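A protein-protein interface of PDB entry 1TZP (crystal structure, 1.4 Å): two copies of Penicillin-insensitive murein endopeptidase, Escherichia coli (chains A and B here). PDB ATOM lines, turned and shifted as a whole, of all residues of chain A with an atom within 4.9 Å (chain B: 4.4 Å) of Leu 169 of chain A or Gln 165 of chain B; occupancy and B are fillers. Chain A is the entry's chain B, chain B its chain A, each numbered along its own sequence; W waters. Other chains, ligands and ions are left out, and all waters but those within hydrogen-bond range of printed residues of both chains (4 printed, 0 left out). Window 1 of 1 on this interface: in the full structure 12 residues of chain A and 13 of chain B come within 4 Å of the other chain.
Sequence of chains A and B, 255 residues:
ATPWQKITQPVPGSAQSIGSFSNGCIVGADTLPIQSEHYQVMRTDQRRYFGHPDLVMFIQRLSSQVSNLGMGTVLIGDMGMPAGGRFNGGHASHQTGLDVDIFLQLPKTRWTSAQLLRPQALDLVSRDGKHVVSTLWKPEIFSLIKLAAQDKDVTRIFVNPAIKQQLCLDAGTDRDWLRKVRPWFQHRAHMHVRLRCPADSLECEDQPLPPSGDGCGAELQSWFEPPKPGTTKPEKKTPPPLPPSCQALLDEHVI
Leu 169 of chain A touches just these residues of chain B: Gln 165, Cys 168, Leu 169, Cys 216 and Gly 217. Gln 165 of chain B touches just one residue of chain A: Leu 169 (3.5 Å). Of the printed residues of chain A, Cys 168 of chain B touches Leu 169. Printed residues of chain A within 4 Å of Gly 217 of chain B: Leu 169 (3.7 Å) and Asp 170 (3.6 Å). Leu 220 of chain B touches none of the printed residues of chain A. The nearest printed residue of chain B that does not touch Leu 169 of chain A is Leu 220 of chain B (4.7 Å). The nearest printed residue of chain A that does not touch Gln 165 of chain B is Gln 166 of chain A (5.2 Å). The nearest printed residue of chain A that does not touch Gly 217 of chain B is Gln 166 of chain A (4.9 Å).
The backbone carbonyl oxygen (O) of Lys 130 of chain B lies within hydrogen-bond range of the side-chain amide nitrogen (NE2) of Gln 165 of chain B, at 3.0 Å. The side-chain sulfur (SG) of Cys 216 of chain B is disulfide-bonded to the side-chain sulfur (SG) of Cys 168 of chain B (2.0 Å). OD1 of Asp 170 of chain A sits at hydrogen-bond distance from NE2 of Gln 166 of chain A.
Gln 165 of chain A touches Leu 169 of chain B. Leu 169 of chain B touches Cys 168 of chain A (CD2 to CB, 3.6 Å). Gln 165 of chain B touches Leu 169 of chain A. Leu 169 of chain A touches Cys 168 of chain B. Leu 169 of chain B touches Leu 169 of chain A. O of Leu 169 of chain A touches CB of Cys 216 of chain B (3.2 Å). Leu 169 of chain A touches Gly 217 of chain B (O to N, 3.7 Å). Gly 217 of chain B touches Asp 170 of chain A (CA to OD1, 3.6 Å).
Water W4 lies within hydrogen-bond range of the side-chain carboxylate (OD1) of Asp 170 of chain A, the backbone carbonyl oxygen (O) of Gly 217 of chain B and the side-chain amide nitrogen (NE2) of Gln 166 of chain A. Water W3 lies within hydrogen-bond range of the backbone carbonyl oxygen (O) of Cys 216 of chain B (2.7 Å), the backbone carbonyl oxygen (O) of Gly 217 of chain B (2.9 Å) and the side-chain amide nitrogen (NE2) of Gln 166 of chain A (2.9 Å). Water W1 bridges the backbone carbonyl oxygen of Leu 169 of chain A (2.9 Å) and the backbone NH of Gly 217 of chain B (3.5 Å). Water W2 lies within hydrogen-bond range of the side-chain amide nitrogen of Gln 165 of chain A and the backbone carbonyl oxygen of Lys 130 of chain B.
Printed residues of chain A that touch a printed residue of chain B: Gln 165, Cys 168, Leu 169 and Asp 170. Hydrophobic or aromatic side chains of chain A within 4 Å of the printed part of chain B: Leu 169. Printed residues of chain B that touch a printed residue of chain A: Gln 165, Cys 168, Leu 169, Cys 216 and Gly 217.
Gln 165 of chain A touches Leu 169 of chain B, and with the chains exchanged Leu 169 of chain A touches Gln 165 of chain B. Cys 168 of chain A touches Leu 169 of chain B, and with the chains exchanged Leu 169 of chain A touches Cys 168 of chain B. Leu 169 of chain A touches its own counterpart, Leu 169 of chain B.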
ATOM      1  N   GLN A 165      31.370 -11.588  10.220  1.00  0.00           N
ATOM      2  CA  GLN A 165      31.113 -11.559   8.782  1.00  0.00           C
ATOM      3  C   GLN A 165      29.639 -11.838   8.528  1.00  0.00           C
ATOM      4  O   GLN A 165      28.999 -11.139   7.717  1.00  0.00           O
ATOM      5  CB  GLN A 165      32.026 -12.580   8.109  1.00  0.00           C
ATOM      6  CG  GLN A 165      31.902 -12.627   6.596  1.00  0.00           C
ATOM      7  CD  GLN A 165      33.017 -13.391   5.977  1.00  0.00           C
ATOM      8  OE1 GLN A 165      33.859 -12.821   5.303  1.00  0.00           O
ATOM      9  NE2 GLN A 165      33.052 -14.677   6.242  1.00  0.00           N
ATOM     10  N   GLN A 166      29.066 -12.814   9.206  1.00  0.00           N
ATOM     11  CA  GLN A 166      27.673 -13.150   8.994  1.00  0.00           C
ATOM     12  C   GLN A 166      26.749 -12.039   9.495  1.00  0.00           C
ATOM     13  O   GLN A 166      25.724 -11.755   8.868  1.00  0.00           O
ATOM     14  CB  GLN A 166      27.307 -14.496   9.616  1.00  0.00           C
ATOM     15  CG  GLN A 166      25.923 -14.970   9.246  1.00  0.00           C
ATOM     16  CD  GLN A 166      25.780 -15.280   7.741  1.00  0.00           C
ATOM     17  OE1 GLN A 166      26.620 -15.980   7.170  1.00  0.00           O
ATOM     18  NE2 GLN A 166      24.751 -14.716   7.093  1.00  0.00           N
ATOM     19  N   LEU A 167      27.089 -11.398  10.609  1.00  0.00           N
ATOM     20  CA  LEU A 167      26.303 -10.276  11.090  1.00  0.00           C
ATOM     21  C   LEU A 167      26.315  -9.133  10.072  1.00  0.00           C
ATOM     22  O   LEU A 167      25.306  -8.467   9.850  1.00  0.00           O
ATOM     23  CB  LEU A 167      26.850  -9.823  12.448  1.00  0.00           C
ATOM     24  CG  LEU A 167      26.724 -10.820  13.620  1.00  0.00           C
ATOM     25  CD1 LEU A 167      27.524 -10.345  14.791  1.00  0.00           C
ATOM     26  CD2 LEU A 167      25.280 -11.018  14.025  1.00  0.00           C
ATOM     27  N   CYS A 168      27.452  -8.914   9.418  1.00  0.00           N
ATOM     28  CA  CYS A 168      27.577  -7.897   8.397  1.00  0.00           C
ATOM     29  C   CYS A 168      26.623  -8.194   7.231  1.00  0.00           C
ATOM     30  O   CYS A 168      26.072  -7.258   6.619  1.00  0.00           O
ATOM     31  CB  CYS A 168      29.017  -7.878   7.881  1.00  0.00           C
ATOM     32  SG  CYS A 168      30.226  -7.136   8.971  1.00  0.00           S
ATOM     33  N   LEU A 169      26.440  -9.467   6.892  1.00  0.00           N
ATOM     34  CA  LEU A 169      25.543  -9.884   5.814  1.00  0.00           C
ATOM     35  C   LEU A 169      24.075  -9.729   6.234  1.00  0.00           C
ATOM     36  O   LEU A 169      23.235  -9.334   5.423  1.00  0.00           O
ATOM     37  CB  LEU A 169      25.823 -11.329   5.399  1.00  0.00           C
ATOM     38  CG  LEU A 169      27.207 -11.608   4.817  1.00  0.00           C
ATOM     39  CD1 LEU A 169      27.413 -13.048   4.601  1.00  0.00           C
ATOM     40  CD2 LEU A 169      27.420 -10.805   3.555  1.00  0.00           C
ATOM     41  N   ASP A 170      23.731 -10.049   7.480  1.00  0.00           N
ATOM     42  CA  ASP A 170      22.341 -10.085   7.928  1.00  0.00           C
ATOM     43  C   ASP A 170      21.794  -8.700   8.253  1.00  0.00           C
ATOM     44  O   ASP A 170      20.578  -8.577   8.405  1.00  0.00           O
ATOM     45  CB  ASP A 170      22.238 -10.918   9.209  1.00  0.00           C
ATOM     46  CG  ASP A 170      22.413 -12.401   9.001  1.00  0.00           C
ATOM     47  OD1 ASP A 170      22.569 -12.904   7.857  1.00  0.00           O
ATOM     48  OD2 ASP A 170      22.352 -13.159   9.999  1.00  0.00           O
ATOM     49  N   ALA A 171      22.637  -7.692   8.442  1.00  0.00           N
ATOM     50  CA  ALA A 171      22.202  -6.447   9.089  1.00  0.00           C
ATOM     51  C   ALA A 171      21.314  -5.546   8.264  1.00  0.00           C
ATOM     52  O   ALA A 171      20.548  -4.750   8.826  1.00  0.00           O
ATOM     53  CB  ALA A 171      23.379  -5.649   9.580  1.00  0.00           C
ATOM     54  N   GLY A 172      21.383  -5.654   6.949  1.00  0.00           N
ATOM     55  CA  GLY A 172      20.561  -4.797   6.099  1.00  0.00           C
ATOM     56  C   GLY A 172      20.929  -3.342   6.210  1.00  0.00           C
ATOM     57  O   GLY A 172      22.097  -3.012   6.192  1.00  0.00           O
ATOM     58  N   LYS B 130      32.915 -21.249  -1.277  1.00  0.00           N
ATOM     59  CA  LYS B 130      32.459 -20.561  -0.073  1.00  0.00           C
ATOM     60  C   LYS B 130      32.781 -19.079  -0.038  1.00  0.00           C
ATOM     61  O   LYS B 130      32.093 -18.341   0.635  1.00  0.00           O
ATOM     62  CB  LYS B 130      33.012 -21.251   1.197  1.00  0.00           C
ATOM     63  CG  LYS B 130      32.537 -22.707   1.446  1.00  0.00           C
ATOM     64  CD  LYS B 130      31.042 -22.759   1.728  1.00  0.00           C
ATOM     65  CE  LYS B 130      30.524 -24.082   2.289  1.00  0.00           C
ATOM     66  NZ  LYS B 130      29.120 -23.893   2.854  1.00  0.00           N
ATOM     67  N   HIS B 131      33.810 -18.621  -0.759  1.00  0.00           N
ATOM     68  CA  HIS B 131      34.226 -17.216  -0.716  1.00  0.00           C
ATOM     69  C   HIS B 131      34.985 -16.820  -1.975  1.00  0.00           C
ATOM     70  O   HIS B 131      35.543 -17.676  -2.682  1.00  0.00           O
ATOM     71  CB  HIS B 131      35.092 -16.928   0.517  1.00  0.00           C
ATOM     72  CG  HIS B 131      36.300 -17.808   0.604  1.00  0.00           C
ATOM     73  ND1 HIS B 131      37.493 -17.511  -0.020  1.00  0.00           N
ATOM     74  CD2 HIS B 131      36.487 -19.001   1.218  1.00  0.00           C
ATOM     75  CE1 HIS B 131      38.362 -18.478   0.216  1.00  0.00           C
ATOM     76  NE2 HIS B 131      37.774 -19.399   0.954  1.00  0.00           N
ATOM     77  N   PRO B 161      27.025 -17.067  -5.785  1.00  0.00           N
ATOM     78  CA  PRO B 161      26.725 -16.605  -4.431  1.00  0.00           C
ATOM     79  C   PRO B 161      27.929 -16.005  -3.694  1.00  0.00           C
ATOM     80  O   PRO B 161      27.799 -15.052  -2.936  1.00  0.00           O
ATOM     81  CB  PRO B 161      26.205 -17.855  -3.717  1.00  0.00           C
ATOM     82  CG  PRO B 161      25.816 -18.803  -4.784  1.00  0.00           C
ATOM     83  CD  PRO B 161      26.595 -18.458  -6.003  1.00  0.00           C
ATOM     84  N   ALA B 162      29.125 -16.573  -3.909  1.00  0.00           N
ATOM     85  CA  ALA B 162      30.312 -16.028  -3.245  1.00  0.00           C
ATOM     86  C   ALA B 162      30.597 -14.618  -3.673  1.00  0.00           C
ATOM     87  O   ALA B 162      31.041 -13.809  -2.894  1.00  0.00           O
ATOM     88  CB  ALA B 162      31.542 -16.886  -3.483  1.00  0.00           C
ATOM     89  N   ILE B 163      30.305 -14.320  -4.944  1.00  0.00           N
ATOM     90  CA  ILE B 163      30.511 -12.964  -5.438  1.00  0.00           C
ATOM     91  C   ILE B 163      29.481 -12.012  -4.821  1.00  0.00           C
ATOM     92  O   ILE B 163      29.858 -10.928  -4.348  1.00  0.00           O
ATOM     93  CB  ILE B 163      30.489 -12.930  -6.977  1.00  0.00           C
ATOM     94  CG1 ILE B 163      31.750 -13.642  -7.521  1.00  0.00           C
ATOM     95  CG2 ILE B 163      30.429 -11.481  -7.478  1.00  0.00           C
ATOM     96  CD1 ILE B 163      31.751 -13.852  -9.039  1.00  0.00           C
ATOM     97  N   LYS B 164      28.207 -12.420  -4.758  1.00  0.00           N
ATOM     98  CA  LYS B 164      27.236 -11.564  -4.053  1.00  0.00           C
ATOM     99  C   LYS B 164      27.638 -11.321  -2.591  1.00  0.00           C
ATOM    100  O   LYS B 164      27.524 -10.218  -2.076  1.00  0.00           O
ATOM    101  CB  LYS B 164      25.793 -12.057  -4.134  1.00  0.00           C
ATOM    102  CG  LYS B 164      24.848 -11.055  -3.463  1.00  0.00           C
ATOM    103  CD  LYS B 164      23.370 -11.246  -3.615  1.00  0.00           C
ATOM    104  CE  LYS B 164      22.597 -10.048  -3.014  1.00  0.00           C
ATOM    105  NZ  LYS B 164      21.109 -10.154  -3.325  1.00  0.00           N
ATOM    106  N   GLN B 165      28.142 -12.362  -1.934  1.00  0.00           N
ATOM    107  CA  GLN B 165      28.592 -12.216  -0.561  1.00  0.00           C
ATOM    108  C   GLN B 165      29.643 -11.117  -0.412  1.00  0.00           C
ATOM    109  O   GLN B 165      29.534 -10.265   0.480  1.00  0.00           O
ATOM    110  CB  GLN B 165      29.143 -13.522  -0.062  1.00  0.00           C
ATOM    111  CG  GLN B 165      29.628 -13.523   1.367  1.00  0.00           C
ATOM    112  CD  GLN B 165      29.747 -14.961   1.827  1.00  0.00           C
ATOM    113  OE1 GLN B 165      28.911 -15.435   2.541  1.00  0.00           O
ATOM    114  NE2 GLN B 165      30.727 -15.699   1.268  1.00  0.00           N
ATOM    115  N   GLN B 166      30.644 -11.090  -1.293  1.00  0.00           N
ATOM    116  CA  GLN B 166      31.645 -10.026  -1.177  1.00  0.00           C
ATOM    117  C   GLN B 166      31.081  -8.653  -1.488  1.00  0.00           C
ATOM    118  O   GLN B 166      31.452  -7.660  -0.849  1.00  0.00           O
ATOM    119  CB  GLN B 166      32.900 -10.311  -1.983  1.00  0.00           C
ATOM    120  CG  GLN B 166      34.083  -9.440  -1.521  1.00  0.00           C
ATOM    121  CD  GLN B 166      34.401  -9.646  -0.028  1.00  0.00           C
ATOM    122  OE1 GLN B 166      34.591 -10.760   0.416  1.00  0.00           O
ATOM    123  NE2 GLN B 166      34.452  -8.568   0.732  1.00  0.00           N
ATOM    124  N   LEU B 167      30.205  -8.579  -2.482  1.00  0.00           N
ATOM    125  CA  LEU B 167      29.520  -7.320  -2.777  1.00  0.00           C
ATOM    126  C   LEU B 167      28.776  -6.790  -1.546  1.00  0.00           C
ATOM    127  O   LEU B 167      28.830  -5.620  -1.253  1.00  0.00           O
ATOM    128  CB  LEU B 167      28.559  -7.472  -3.945  1.00  0.00           C
ATOM    129  CG  LEU B 167      29.198  -7.844  -5.294  1.00  0.00           C
ATOM    130  CD1 LEU B 167      28.099  -8.183  -6.279  1.00  0.00           C
ATOM    131  CD2 LEU B 167      30.096  -6.781  -5.871  1.00  0.00           C
ATOM    132  N   CYS B 168      28.093  -7.705  -0.868  1.00  0.00           N
ATOM    133  CA  CYS B 168      27.353  -7.404   0.368  1.00  0.00           C
ATOM    134  C   CYS B 168      28.272  -6.810   1.440  1.00  0.00           C
ATOM    135  O   CYS B 168      27.901  -5.837   2.124  1.00  0.00           O
ATOM    136  CB  CYS B 168      26.661  -8.665   0.895  1.00  0.00           C
ATOM    137  SG  CYS B 168      25.251  -9.148  -0.117  1.00  0.00           S
ATOM    138  N   LEU B 169      29.458  -7.401   1.610  1.00  0.00           N
ATOM    139  CA  LEU B 169      30.390  -6.893   2.600  1.00  0.00           C
ATOM    140  C   LEU B 169      31.000  -5.551   2.257  1.00  0.00           C
ATOM    141  O   LEU B 169      31.268  -4.718   3.149  1.00  0.00           O
ATOM    142  CB  LEU B 169      31.488  -7.928   2.859  1.00  0.00           C
ATOM    143  CG  LEU B 169      31.047  -9.268   3.443  1.00  0.00           C
ATOM    144  CD1 LEU B 169      32.204 -10.249   3.486  1.00  0.00           C
ATOM    145  CD2 LEU B 169      30.448  -9.112   4.828  1.00  0.00           C
ATOM    146  N   CYS B 216      21.176 -10.132   1.335  1.00  0.00           N
ATOM    147  CA  CYS B 216      22.478 -10.596   1.797  1.00  0.00           C
ATOM    148  C   CYS B 216      22.402 -11.569   2.945  1.00  0.00           C
ATOM    149  O   CYS B 216      23.415 -12.137   3.286  1.00  0.00           O
ATOM    150  CB  CYS B 216      23.334  -9.424   2.210  1.00  0.00           C
ATOM    151  SG  CYS B 216      23.688  -8.275   0.865  1.00  0.00           S
ATOM    152  N   GLY B 217      21.208 -11.751   3.509  1.00  0.00           N
ATOM    153  CA  GLY B 217      20.971 -12.617   4.659  1.00  0.00           C
ATOM    154  C   GLY B 217      20.487 -13.998   4.311  1.00  0.00           C
ATOM    155  O   GLY B 217      21.191 -14.791   3.684  1.00  0.00           O
ATOM    156  N   LEU B 220      20.759 -15.592   0.641  1.00  0.00           N
ATOM    157  CA  LEU B 220      22.142 -15.857   0.286  1.00  0.00           C
ATOM    158  C   LEU B 220      22.697 -17.060   1.034  1.00  0.00           C
ATOM    159  O   LEU B 220      23.348 -17.903   0.437  1.00  0.00           O
ATOM    160  CB  LEU B 220      22.989 -14.630   0.530  1.00  0.00           C
ATOM    161  CG  LEU B 220      24.447 -14.739   0.082  1.00  0.00           C
ATOM    162  CD1 LEU B 220      24.644 -15.131  -1.404  1.00  0.00           C
ATOM    163  CD2 LEU B 220      25.155 -13.436   0.390  1.00  0.00           C
ATOM    164  N   PHE B 224      24.521 -21.537   0.298  1.00  0.00           N
ATOM    165  CA  PHE B 224      25.693 -22.202   0.857  1.00  0.00           C
ATOM    166  C   PHE B 224      25.362 -23.466   1.660  1.00  0.00           C
ATOM    167  O   PHE B 224      26.264 -24.097   2.216  1.00  0.00           O
ATOM    168  CB  PHE B 224      26.479 -21.200   1.710  1.00  0.00           C
ATOM    169  CG  PHE B 224      27.083 -20.075   0.913  1.00  0.00           C
ATOM    170  CD1 PHE B 224      28.047 -20.322  -0.050  1.00  0.00           C
ATOM    171  CD2 PHE B 224      26.683 -18.782   1.131  1.00  0.00           C
ATOM    172  CE1 PHE B 224      28.580 -19.288  -0.774  1.00  0.00           C
ATOM    173  CE2 PHE B 224      27.213 -17.759   0.426  1.00  0.00           C
ATOM    174  CZ  PHE B 224      28.182 -18.005  -0.520  1.00  0.00           C
HETATM  175  O   HOH W   1      20.502  -8.597   4.851  1.00  0.00           O
HETATM  176  O   HOH W   2      33.047 -16.860   3.654  1.00  0.00           O
HETATM  177  O   HOH W   3      24.024 -14.627   4.276  1.00  0.00           O
HETATM  178  O   HOH W   4      21.293 -15.089   7.103  1.00  0.00           O
